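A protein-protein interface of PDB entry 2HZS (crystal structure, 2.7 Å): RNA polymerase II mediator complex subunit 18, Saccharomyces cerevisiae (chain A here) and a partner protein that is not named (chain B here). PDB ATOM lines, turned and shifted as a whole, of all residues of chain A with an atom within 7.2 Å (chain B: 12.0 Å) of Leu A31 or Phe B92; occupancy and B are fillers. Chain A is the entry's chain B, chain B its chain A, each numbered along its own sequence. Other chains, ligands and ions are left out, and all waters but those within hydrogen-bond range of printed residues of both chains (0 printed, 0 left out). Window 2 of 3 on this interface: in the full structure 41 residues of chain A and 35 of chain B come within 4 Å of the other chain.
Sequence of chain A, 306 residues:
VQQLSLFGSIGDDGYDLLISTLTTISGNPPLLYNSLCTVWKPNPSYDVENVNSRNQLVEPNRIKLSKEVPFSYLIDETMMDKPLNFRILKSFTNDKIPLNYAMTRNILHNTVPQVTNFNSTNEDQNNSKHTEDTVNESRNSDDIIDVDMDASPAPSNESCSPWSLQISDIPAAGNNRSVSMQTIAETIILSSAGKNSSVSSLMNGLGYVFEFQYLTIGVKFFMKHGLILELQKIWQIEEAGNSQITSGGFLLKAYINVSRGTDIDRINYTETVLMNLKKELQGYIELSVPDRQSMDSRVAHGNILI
Of the 17 printed residues of chain A, 6 touch a printed residue of chain B. Printed residues of chain A that touch a printed residue of chain B: Leu A31, Leu A32, Tyr A33, Asn A34, Glu A68 and Lys A220. Hydrophobic or aromatic side chains of chain A within 4 Å of the printed part of chain B: Leu A31 and Tyr A33. Of the 18 printed residues of chain B, 5 touch a printed residue of chain A. Hydrophobic or aromatic side chains of chain B that line the printed part of chain A: Ala B89, Leu B90 and Phe B92. Among the printed residues, 10 pairs touch across the chains.
Leu A31 touches one residue of chain B. Phe B92 touches just these residues of chain A: Leu A31 (3.8 Å), Leu A32 (3.4 Å), Tyr A33 (3.7 Å) and Lys A220 (2.5 Å). No residue of chain B comes within 4 Å of Pro A29. Pro A30 touches none of the printed residues of chain B. Of the printed residues of chain B, Tyr A33 touches Phe B92 and Asn B93. No residue of chain B comes within 4 Å of Gly A218. No residue of chain B comes within 4 Å of Val A219. Of chain B, only Phe B92 (2.5 Å) comes within 4 Å of Lys A220. No residue of chain B comes within 4 Å of Phe A221. Printed residues of chain B within 4 Å of Glu A68: Ala B89 (3.9 Å), Leu B90 (2.9 Å), Asn B93 (3.2 Å) and Ser B95 (3.8 Å). Of the printed residues of chain A, Leu B90 touches Glu A68 (2.9 Å). Of the printed residues of chain A, Ala B89 touches Glu A68 (3.9 Å). Ala B84 touches none of the printed residues of chain A. Gly B94 touches none of the printed residues of chain A. The nearest residue of chain B that does not touch Leu A31 is Asn B93 (7.8 Å). The nearest printed residue of chain A that does not touch Leu B90 is Lys A220 (7.0 Å).
Phe B92 touches Leu A31 (CE1 to CD1, 3.8 Å). Phe B92 touches Leu A32. CE2 of Phe B92 touches CB of Tyr A33, 3.7 Å away. Tyr A33 touches Asn B93. Ala B89 touches Glu A68. CD2 of Leu B90 touches OE2 of Glu A68 (2.9 Å). Ser B95 touches Glu A68.
O of Gly A218 lies within hydrogen-bond range of N of Tyr A33, 2.8 Å away. The backbone carbonyl oxygen (O) of Leu B90 lies within hydrogen-bond range of the backbone NH (N) of Ser B95, at 3.2 Å. The backbone carbonyl oxygen of Leu A31 is in hydrogen-bond range of the backbone NH of Lys A220 (2.9 Å). The backbone carbonyl oxygen (O) of Leu B90 is in hydrogen-bond range of the backbone NH (N) of Ser B96 (3.0 Å). The backbone carbonyl oxygen (O) of Leu B90 lies close to the side-chain amide oxygen (OD1) of Asn B93, at 3.1 Å. The side-chain amide nitrogen (ND2) of Asn B93 is in hydrogen-bond range of the side-chain hydroxyl (OG) of Ser B95 (2.8 Å).
The backbone carbonyl oxygen (O) of Phe B92 lies within hydrogen-bond range of the side-chain amino group (NZ) of Lys A220, 2.5 Å away. The side-chain amide nitrogen of Asn B93 sits close to the backbone NH of Glu A68. The side-chain amide nitrogen (ND2) of Asn B93 is in hydrogen-bond range of the backbone carbonyl oxygen (O) of Asn A34, at 2.9 Å.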
ATOM      1  N   ASN A  28      30.362 -14.516 -13.934  1.00  0.00           N
ATOM      2  CA  ASN A  28      29.529 -15.699 -13.702  1.00  0.00           C
ATOM      3  C   ASN A  28      28.405 -15.795 -14.717  1.00  0.00           C
ATOM      4  O   ASN A  28      27.909 -14.777 -15.180  1.00  0.00           O
ATOM      5  CB  ASN A  28      28.875 -15.622 -12.317  1.00  0.00           C
ATOM      6  CG  ASN A  28      29.873 -15.500 -11.188  1.00  0.00           C
ATOM      7  OD1 ASN A  28      30.595 -16.441 -10.883  1.00  0.00           O
ATOM      8  ND2 ASN A  28      29.916 -14.330 -10.558  1.00  0.00           N
ATOM      9  N   PRO A  29      28.006 -17.018 -15.097  1.00  0.00           N
ATOM     10  CA  PRO A  29      26.898 -17.158 -16.053  1.00  0.00           C
ATOM     11  C   PRO A  29      25.605 -16.858 -15.280  1.00  0.00           C
ATOM     12  O   PRO A  29      25.616 -16.786 -14.053  1.00  0.00           O
ATOM     13  CB  PRO A  29      26.995 -18.614 -16.514  1.00  0.00           C
ATOM     14  CG  PRO A  29      27.736 -19.293 -15.402  1.00  0.00           C
ATOM     15  CD  PRO A  29      28.764 -18.272 -14.987  1.00  0.00           C
ATOM     16  N   PRO A  30      24.476 -16.681 -15.975  1.00  0.00           N
ATOM     17  CA  PRO A  30      23.219 -16.375 -15.270  1.00  0.00           C
ATOM     18  C   PRO A  30      22.614 -17.501 -14.405  1.00  0.00           C
ATOM     19  O   PRO A  30      22.882 -18.679 -14.610  1.00  0.00           O
ATOM     20  CB  PRO A  30      22.291 -15.985 -16.417  1.00  0.00           C
ATOM     21  CG  PRO A  30      22.697 -16.980 -17.501  1.00  0.00           C
ATOM     22  CD  PRO A  30      24.235 -16.919 -17.414  1.00  0.00           C
ATOM     23  N   LEU A  31      21.792 -17.117 -13.438  1.00  0.00           N
ATOM     24  CA  LEU A  31      21.105 -18.072 -12.571  1.00  0.00           C
ATOM     25  C   LEU A  31      19.577 -17.944 -12.752  1.00  0.00           C
ATOM     26  O   LEU A  31      18.994 -16.881 -12.491  1.00  0.00           O
ATOM     27  CB  LEU A  31      21.443 -17.797 -11.113  1.00  0.00           C
ATOM     28  CG  LEU A  31      22.892 -17.991 -10.691  1.00  0.00           C
ATOM     29  CD1 LEU A  31      23.090 -17.451  -9.263  1.00  0.00           C
ATOM     30  CD2 LEU A  31      23.238 -19.461 -10.762  1.00  0.00           C
ATOM     31  N   LEU A  32      18.936 -19.026 -13.185  1.00  0.00           N
ATOM     32  CA  LEU A  32      17.481 -19.048 -13.389  1.00  0.00           C
ATOM     33  C   LEU A  32      16.690 -18.892 -12.082  1.00  0.00           C
ATOM     34  O   LEU A  32      17.055 -19.486 -11.060  1.00  0.00           O
ATOM     35  CB  LEU A  32      17.081 -20.365 -14.045  1.00  0.00           C
ATOM     36  CG  LEU A  32      15.592 -20.574 -14.231  1.00  0.00           C
ATOM     37  CD1 LEU A  32      15.081 -19.604 -15.279  1.00  0.00           C
ATOM     38  CD2 LEU A  32      15.346 -22.014 -14.634  1.00  0.00           C
ATOM     39  N   TYR A  33      15.598 -18.126 -12.118  1.00  0.00           N
ATOM     40  CA  TYR A  33      14.778 -17.932 -10.933  1.00  0.00           C
ATOM     41  C   TYR A  33      13.365 -17.483 -11.291  1.00  0.00           C
ATOM     42  O   TYR A  33      13.122 -16.979 -12.393  1.00  0.00           O
ATOM     43  CB  TYR A  33      15.420 -16.883 -10.038  1.00  0.00           C
ATOM     44  CG  TYR A  33      15.073 -15.461 -10.429  1.00  0.00           C
ATOM     45  CD1 TYR A  33      13.905 -14.849  -9.954  1.00  0.00           C
ATOM     46  CD2 TYR A  33      15.889 -14.736 -11.294  1.00  0.00           C
ATOM     47  CE1 TYR A  33      13.566 -13.568 -10.334  1.00  0.00           C
ATOM     48  CE2 TYR A  33      15.551 -13.445 -11.674  1.00  0.00           C
ATOM     49  CZ  TYR A  33      14.389 -12.874 -11.189  1.00  0.00           C
ATOM     50  OH  TYR A  33      14.026 -11.612 -11.581  1.00  0.00           O
ATOM     51  N   ASN A  34      12.428 -17.659 -10.361  1.00  0.00           N
ATOM     52  CA  ASN A  34      11.056 -17.201 -10.585  1.00  0.00           C
ATOM     53  C   ASN A  34      10.438 -16.717  -9.287  1.00  0.00           C
ATOM     54  O   ASN A  34      11.006 -16.907  -8.228  1.00  0.00           O
ATOM     55  CB  ASN A  34      10.175 -18.301 -11.202  1.00  0.00           C
ATOM     56  CG  ASN A  34       9.726 -19.365 -10.200  1.00  0.00           C
ATOM     57  OD1 ASN A  34       9.140 -19.064  -9.167  1.00  0.00           O
ATOM     58  ND2 ASN A  34       9.968 -20.624 -10.536  1.00  0.00           N
ATOM     59  N   GLU A  68       8.641 -18.039  -4.096  1.00  0.00           N
ATOM     60  CA  GLU A  68       9.045 -18.760  -5.296  1.00  0.00           C
ATOM     61  C   GLU A  68       8.094 -19.932  -5.456  1.00  0.00           C
ATOM     62  O   GLU A  68       7.466 -20.374  -4.492  1.00  0.00           O
ATOM     63  CB  GLU A  68      10.457 -19.335  -5.158  1.00  0.00           C
ATOM     64  CG  GLU A  68      10.495 -20.636  -4.352  1.00  0.00           C
ATOM     65  CD  GLU A  68      10.112 -20.423  -2.879  1.00  0.00           C
ATOM     66  OE1 GLU A  68       9.860 -21.421  -2.155  1.00  0.00           O
ATOM     67  OE2 GLU A  68      10.079 -19.251  -2.438  1.00  0.00           O
ATOM     68  N   GLY A 218      13.080 -15.240 -14.784  1.00  0.00           N
ATOM     69  CA  GLY A 218      14.250 -14.583 -15.315  1.00  0.00           C
ATOM     70  C   GLY A 218      15.549 -15.186 -14.838  1.00  0.00           C
ATOM     71  O   GLY A 218      15.576 -16.264 -14.219  1.00  0.00           O
ATOM     72  N   VAL A 219      16.635 -14.499 -15.173  1.00  0.00           N
ATOM     73  CA  VAL A 219      17.958 -14.919 -14.767  1.00  0.00           C
ATOM     74  C   VAL A 219      18.584 -13.763 -13.988  1.00  0.00           C
ATOM     75  O   VAL A 219      18.303 -12.593 -14.272  1.00  0.00           O
ATOM     76  CB  VAL A 219      18.829 -15.249 -15.977  1.00  0.00           C
ATOM     77  CG1 VAL A 219      18.306 -16.485 -16.655  1.00  0.00           C
ATOM     78  CG2 VAL A 219      18.862 -14.069 -16.935  1.00  0.00           C
ATOM     79  N   LYS A 220      19.408 -14.077 -12.994  1.00  0.00           N
ATOM     80  CA  LYS A 220      20.049 -13.016 -12.222  1.00  0.00           C
ATOM     81  C   LYS A 220      21.549 -13.206 -12.188  1.00  0.00           C
ATOM     82  O   LYS A 220      22.049 -14.301 -12.444  1.00  0.00           O
ATOM     83  CB  LYS A 220      19.484 -12.948 -10.789  1.00  0.00           C
ATOM     84  CG  LYS A 220      19.617 -14.223  -9.974  1.00  0.00           C
ATOM     85  CD  LYS A 220      18.794 -14.146  -8.711  1.00  0.00           C
ATOM     86  CE  LYS A 220      19.400 -13.238  -7.662  1.00  0.00           C
ATOM     87  NZ  LYS A 220      18.389 -12.857  -6.625  1.00  0.00           N
ATOM     88  N   PHE A 221      22.256 -12.123 -11.888  1.00  0.00           N
ATOM     89  CA  PHE A 221      23.709 -12.120 -11.817  1.00  0.00           C
ATOM     90  C   PHE A 221      24.132 -11.471 -10.524  1.00  0.00           C
ATOM     91  O   PHE A 221      23.635 -10.388 -10.189  1.00  0.00           O
ATOM     92  CB  PHE A 221      24.327 -11.288 -12.946  1.00  0.00           C
ATOM     93  CG  PHE A 221      24.132 -11.850 -14.316  1.00  0.00           C
ATOM     94  CD1 PHE A 221      23.020 -11.501 -15.075  1.00  0.00           C
ATOM     95  CD2 PHE A 221      25.084 -12.700 -14.871  1.00  0.00           C
ATOM     96  CE1 PHE A 221      22.856 -11.991 -16.380  1.00  0.00           C
ATOM     97  CE2 PHE A 221      24.931 -13.198 -16.175  1.00  0.00           C
ATOM     98  CZ  PHE A 221      23.812 -12.839 -16.927  1.00  0.00           C
ATOM     99  N   PHE A 222      25.040 -12.121  -9.797  1.00  0.00           N
ATOM    100  CA  PHE A 222      25.551 -11.541  -8.563  1.00  0.00           C
ATOM    101  C   PHE A 222      26.838 -10.803  -8.920  1.00  0.00           C
ATOM    102  O   PHE A 222      27.745 -11.368  -9.529  1.00  0.00           O
ATOM    103  CB  PHE A 222      25.861 -12.617  -7.548  1.00  0.00           C
ATOM    104  CG  PHE A 222      24.666 -13.209  -6.923  1.00  0.00           C
ATOM    105  CD1 PHE A 222      23.908 -12.476  -6.029  1.00  0.00           C
ATOM    106  CD2 PHE A 222      24.304 -14.513  -7.200  1.00  0.00           C
ATOM    107  CE1 PHE A 222      22.790 -13.035  -5.408  1.00  0.00           C
ATOM    108  CE2 PHE A 222      23.184 -15.094  -6.588  1.00  0.00           C
ATOM    109  CZ  PHE A 222      22.425 -14.352  -5.686  1.00  0.00           C
ATOM    110  N   ILE A 228      22.940  -6.508  -7.890  1.00  0.00           N
ATOM    111  CA  ILE A 228      22.265  -7.637  -8.515  1.00  0.00           C
ATOM    112  C   ILE A 228      21.587  -7.201  -9.803  1.00  0.00           C
ATOM    113  O   ILE A 228      21.018  -6.111  -9.887  1.00  0.00           O
ATOM    114  CB  ILE A 228      21.242  -8.279  -7.543  1.00  0.00           C
ATOM    115  CG1 ILE A 228      22.015  -8.931  -6.398  1.00  0.00           C
ATOM    116  CG2 ILE A 228      20.420  -9.348  -8.254  1.00  0.00           C
ATOM    117  CD1 ILE A 228      21.329  -9.004  -5.163  1.00  0.00           C
ATOM    118  N   LEU A 229      21.677  -8.054 -10.813  1.00  0.00           N
ATOM    119  CA  LEU A 229      21.101  -7.758 -12.107  1.00  0.00           C
ATOM    120  C   LEU A 229      20.105  -8.820 -12.483  1.00  0.00           C
ATOM    121  O   LEU A 229      20.429  -9.998 -12.482  1.00  0.00           O
ATOM    122  CB  LEU A 229      22.200  -7.690 -13.154  1.00  0.00           C
ATOM    123  CG  LEU A 229      22.627  -6.263 -13.478  1.00  0.00           C
ATOM    124  CD1 LEU A 229      24.134  -6.174 -13.580  1.00  0.00           C
ATOM    125  CD2 LEU A 229      21.936  -5.821 -14.776  1.00  0.00           C
ATOM    126  N   GLU A 230      18.881  -8.397 -12.787  1.00  0.00           N
ATOM    127  CA  GLU A 230      17.827  -9.325 -13.171  1.00  0.00           C
ATOM    128  C   GLU A 230      17.335  -9.029 -14.575  1.00  0.00           C
ATOM    129  O   GLU A 230      17.107  -7.881 -14.944  1.00  0.00           O
ATOM    130  CB  GLU A 230      16.645  -9.245 -12.200  1.00  0.00           C
ATOM    131  CG  GLU A 230      16.986  -9.515 -10.752  1.00  0.00           C
ATOM    132  CD  GLU A 230      15.782  -9.407  -9.827  1.00  0.00           C
ATOM    133  OE1 GLU A 230      14.934  -8.511 -10.033  1.00  0.00           O
ATOM    134  OE2 GLU A 230      15.683 -10.215  -8.882  1.00  0.00           O
ATOM    135  N   TYR A 255      20.036  -3.401  -9.048  1.00  0.00           N
ATOM    136  CA  TYR A 255      19.691  -2.815  -7.762  1.00  0.00           C
ATOM    137  C   TYR A 255      20.556  -3.288  -6.620  1.00  0.00           C
ATOM    138  O   TYR A 255      21.244  -4.302  -6.725  1.00  0.00           O
ATOM    139  CB  TYR A 255      18.233  -3.157  -7.435  1.00  0.00           C
ATOM    140  CG  TYR A 255      18.041  -4.608  -7.034  1.00  0.00           C
ATOM    141  CD1 TYR A 255      18.134  -4.999  -5.691  1.00  0.00           C
ATOM    142  CD2 TYR A 255      17.806  -5.599  -7.990  1.00  0.00           C
ATOM    143  CE1 TYR A 255      18.001  -6.331  -5.308  1.00  0.00           C
ATOM    144  CE2 TYR A 255      17.674  -6.943  -7.617  1.00  0.00           C
ATOM    145  CZ  TYR A 255      17.775  -7.295  -6.270  1.00  0.00           C
ATOM    146  OH  TYR A 255      17.682  -8.611  -5.886  1.00  0.00           O
ATOM    147  N   ALA B  83      16.340 -11.576   9.695  1.00  0.00           N
ATOM    148  CA  ALA B  83      16.863 -11.907   8.385  1.00  0.00           C
ATOM    149  C   ALA B  83      17.396 -13.348   8.380  1.00  0.00           C
ATOM    150  O   ALA B  83      17.345 -14.037   7.366  1.00  0.00           O
ATOM    151  CB  ALA B  83      17.961 -10.932   8.001  1.00  0.00           C
ATOM    152  N   ALA B  84      17.884 -13.811   9.525  1.00  0.00           N
ATOM    153  CA  ALA B  84      18.433 -15.156   9.616  1.00  0.00           C
ATOM    154  C   ALA B  84      17.385 -16.256   9.496  1.00  0.00           C
ATOM    155  O   ALA B  84      17.709 -17.410   9.231  1.00  0.00           O
ATOM    156  CB  ALA B  84      19.185 -15.311  10.916  1.00  0.00           C
ATOM    157  N   ASP B  85      16.125 -15.907   9.708  1.00  0.00           N
ATOM    158  CA  ASP B  85      15.058 -16.890   9.609  1.00  0.00           C
ATOM    159  C   ASP B  85      14.376 -16.954   8.247  1.00  0.00           C
ATOM    160  O   ASP B  85      13.430 -17.736   8.063  1.00  0.00           O
ATOM    161  CB  ASP B  85      13.990 -16.620  10.660  1.00  0.00           C
ATOM    162  CG  ASP B  85      14.465 -16.901  12.069  1.00  0.00           C
ATOM    163  OD1 ASP B  85      15.401 -17.707  12.260  1.00  0.00           O
ATOM    164  OD2 ASP B  85      13.868 -16.324  12.990  1.00  0.00           O
ATOM    165  N   ILE B  86      14.843 -16.143   7.299  1.00  0.00           N
ATOM    166  CA  ILE B  86      14.251 -16.139   5.971  1.00  0.00           C
ATOM    167  C   ILE B  86      14.577 -17.415   5.201  1.00  0.00           C
ATOM    168  O   ILE B  86      15.734 -17.815   5.104  1.00  0.00           O
ATOM    169  CB  ILE B  86      14.754 -14.962   5.117  1.00  0.00           C
ATOM    170  CG1 ILE B  86      14.644 -13.642   5.879  1.00  0.00           C
ATOM    171  CG2 ILE B  86      13.934 -14.879   3.872  1.00  0.00           C
ATOM    172  CD1 ILE B  86      15.290 -12.452   5.161  1.00  0.00           C
ATOM    173  N   PRO B  87      13.556 -18.087   4.662  1.00  0.00           N
ATOM    174  CA  PRO B  87      13.812 -19.309   3.896  1.00  0.00           C
ATOM    175  C   PRO B  87      14.797 -18.942   2.789  1.00  0.00           C
ATOM    176  O   PRO B  87      14.587 -17.975   2.056  1.00  0.00           O
ATOM    177  CB  PRO B  87      12.439 -19.653   3.347  1.00  0.00           C
ATOM    178  CG  PRO B  87      11.542 -19.221   4.458  1.00  0.00           C
ATOM    179  CD  PRO B  87      12.116 -17.887   4.885  1.00  0.00           C
ATOM    180  N   PRO B  88      15.900 -19.693   2.664  1.00  0.00           N
ATOM    181  CA  PRO B  88      16.893 -19.398   1.623  1.00  0.00           C
ATOM    182  C   PRO B  88      16.331 -19.144   0.224  1.00  0.00           C
ATOM    183  O   PRO B  88      16.756 -18.212  -0.463  1.00  0.00           O
ATOM    184  CB  PRO B  88      17.798 -20.615   1.674  1.00  0.00           C
ATOM    185  CG  PRO B  88      17.780 -20.928   3.153  1.00  0.00           C
ATOM    186  CD  PRO B  88      16.331 -20.838   3.487  1.00  0.00           C
ATOM    187  N   ALA B  89      15.368 -19.949  -0.199  1.00  0.00           N
ATOM    188  CA  ALA B  89      14.831 -19.764  -1.536  1.00  0.00           C
ATOM    189  C   ALA B  89      14.211 -18.382  -1.764  1.00  0.00           C
ATOM    190  O   ALA B  89      14.316 -17.843  -2.865  1.00  0.00           O
ATOM    191  CB  ALA B  89      13.820 -20.861  -1.870  1.00  0.00           C
ATOM    192  N   LEU B  90      13.588 -17.796  -0.743  1.00  0.00           N
ATOM    193  CA  LEU B  90      12.976 -16.484  -0.915  1.00  0.00           C
ATOM    194  C   LEU B  90      14.003 -15.388  -1.086  1.00  0.00           C
ATOM    195  O   LEU B  90      13.705 -14.346  -1.669  1.00  0.00           O
ATOM    196  CB  LEU B  90      12.056 -16.132   0.256  1.00  0.00           C
ATOM    197  CG  LEU B  90      10.761 -16.933   0.367  1.00  0.00           C
ATOM    198  CD1 LEU B  90      10.003 -16.474   1.592  1.00  0.00           C
ATOM    199  CD2 LEU B  90       9.920 -16.764  -0.869  1.00  0.00           C
ATOM    200  N   VAL B  91      15.205 -15.601  -0.570  1.00  0.00           N
ATOM    201  CA  VAL B  91      16.250 -14.595  -0.715  1.00  0.00           C
ATOM    202  C   VAL B  91      16.841 -14.706  -2.111  1.00  0.00           C
ATOM    203  O   VAL B  91      17.129 -13.702  -2.764  1.00  0.00           O
ATOM    204  CB  VAL B  91      17.386 -14.788   0.324  1.00  0.00           C
ATOM    205  CG1 VAL B  91      18.549 -13.840   0.026  1.00  0.00           C
ATOM    206  CG2 VAL B  91      16.851 -14.504   1.721  1.00  0.00           C
ATOM    207  N   PHE B  92      16.988 -15.938  -2.581  1.00  0.00           N
ATOM    208  CA  PHE B  92      17.538 -16.146  -3.903  1.00  0.00           C
ATOM    209  C   PHE B  92      16.742 -15.605  -5.088  1.00  0.00           C
ATOM    210  O   PHE B  92      17.335 -15.054  -6.014  1.00  0.00           O
ATOM    211  CB  PHE B  92      17.802 -17.617  -4.149  1.00  0.00           C
ATOM    212  CG  PHE B  92      18.194 -17.906  -5.555  1.00  0.00           C
ATOM    213  CD1 PHE B  92      19.415 -17.445  -6.062  1.00  0.00           C
ATOM    214  CD2 PHE B  92      17.305 -18.558  -6.413  1.00  0.00           C
ATOM    215  CE1 PHE B  92      19.733 -17.625  -7.402  1.00  0.00           C
ATOM    216  CE2 PHE B  92      17.614 -18.741  -7.748  1.00  0.00           C
ATOM    217  CZ  PHE B  92      18.829 -18.273  -8.248  1.00  0.00           C
ATOM    218  N   ASN B  93      15.423 -15.752  -5.073  1.00  0.00           N
ATOM    219  CA  ASN B  93      14.616 -15.304  -6.205  1.00  0.00           C
ATOM    220  C   ASN B  93      14.134 -13.872  -6.101  1.00  0.00           C
ATOM    221  O   ASN B  93      13.392 -13.391  -6.979  1.00  0.00           O
ATOM    222  CB  ASN B  93      13.430 -16.230  -6.384  1.00  0.00           C
ATOM    223  CG  ASN B  93      12.549 -16.223  -5.196  1.00  0.00           C
ATOM    224  OD1 ASN B  93      13.035 -16.225  -4.087  1.00  0.00           O
ATOM    225  ND2 ASN B  93      11.254 -16.213  -5.404  1.00  0.00           N
ATOM    226  N   GLY B  94      14.558 -13.195  -5.035  1.00  0.00           N
ATOM    227  CA  GLY B  94      14.187 -11.805  -4.853  1.00  0.00           C
ATOM    228  C   GLY B  94      12.826 -11.544  -4.239  1.00  0.00           C
ATOM    229  O   GLY B  94      12.432 -10.384  -4.140  1.00  0.00           O
ATOM    230  N   SER B  95      12.101 -12.588  -3.828  1.00  0.00           N
ATOM    231  CA  SER B  95      10.793 -12.376  -3.207  1.00  0.00           C
ATOM    232  C   SER B  95      11.006 -11.537  -1.952  1.00  0.00           C
ATOM    233  O   SER B  95      10.203 -10.666  -1.620  1.00  0.00           O
ATOM    234  CB  SER B  95      10.124 -13.700  -2.828  1.00  0.00           C
ATOM    235  OG  SER B  95       9.721 -14.424  -3.971  1.00  0.00           O
ATOM    236  N   SER B  96      12.109 -11.801  -1.260  1.00  0.00           N
ATOM    237  CA  SER B  96      12.441 -11.069  -0.048  1.00  0.00           C
ATOM    238  C   SER B  96      13.616 -10.120  -0.313  1.00  0.00           C
ATOM    239  O   SER B  96      14.420 -10.362  -1.215  1.00  0.00           O
ATOM    240  CB  SER B  96      12.811 -12.049   1.054  1.00  0.00           C
ATOM    241  OG  SER B  96      13.301 -11.370   2.189  1.00  0.00           O
ATOM    242  N   THR B  97      13.706  -9.036   0.454  1.00  0.00           N
ATOM    243  CA  THR B  97      14.790  -8.073   0.278  1.00  0.00           C
ATOM    244  C   THR B  97      15.959  -8.488   1.147  1.00  0.00           C
ATOM    245  O   THR B  97      17.035  -7.893   1.085  1.00  0.00           O
ATOM    246  CB  THR B  97      14.404  -6.669   0.743  1.00  0.00           C
ATOM    247  OG1 THR B  97      14.024  -6.728   2.128  1.00  0.00           O
ATOM    248  CG2 THR B  97      13.271  -6.093  -0.109  1.00  0.00           C
ATOM    249  N   GLY B  98      15.731  -9.501   1.975  1.00  0.00           N
ATOM    250  CA  GLY B  98      16.769  -9.977   2.864  1.00  0.00           C
ATOM    251  C   GLY B  98      16.839  -9.130   4.126  1.00  0.00           C
ATOM    252  O   GLY B  98      17.596  -9.436   5.042  1.00  0.00           O
ATOM    253  N   VAL B  99      16.038  -8.073   4.194  1.00  0.00           N
ATOM    254  CA  VAL B  99      16.057  -7.194   5.361  1.00  0.00           C
ATOM    255  C   VAL B  99      14.646  -6.929   5.896  1.00  0.00           C
ATOM    256  O   VAL B  99      14.074  -5.849   5.693  1.00  0.00           O
ATOM    257  CB  VAL B  99      16.697  -5.848   4.992  1.00  0.00           C
ATOM    258  CG1 VAL B  99      16.962  -5.025   6.242  1.00  0.00           C
ATOM    259  CG2 VAL B  99      17.961  -6.088   4.165  1.00  0.00           C
ATOM    260  N   PRO B 100      14.068  -7.912   6.595  1.00  0.00           N
ATOM    261  CA  PRO B 100      12.717  -7.779   7.149  1.00  0.00           C
ATOM    262  C   PRO B 100      12.648  -7.010   8.459  1.00  0.00           C
ATOM    263  O   PRO B 100      13.670  -6.742   9.084  1.00  0.00           O
ATOM    264  CB  PRO B 100      12.295  -9.225   7.335  1.00  0.00           C
ATOM    265  CG  PRO B 100      13.579  -9.869   7.781  1.00  0.00           C
ATOM    266  CD  PRO B 100      14.597  -9.271   6.821  1.00  0.00           C
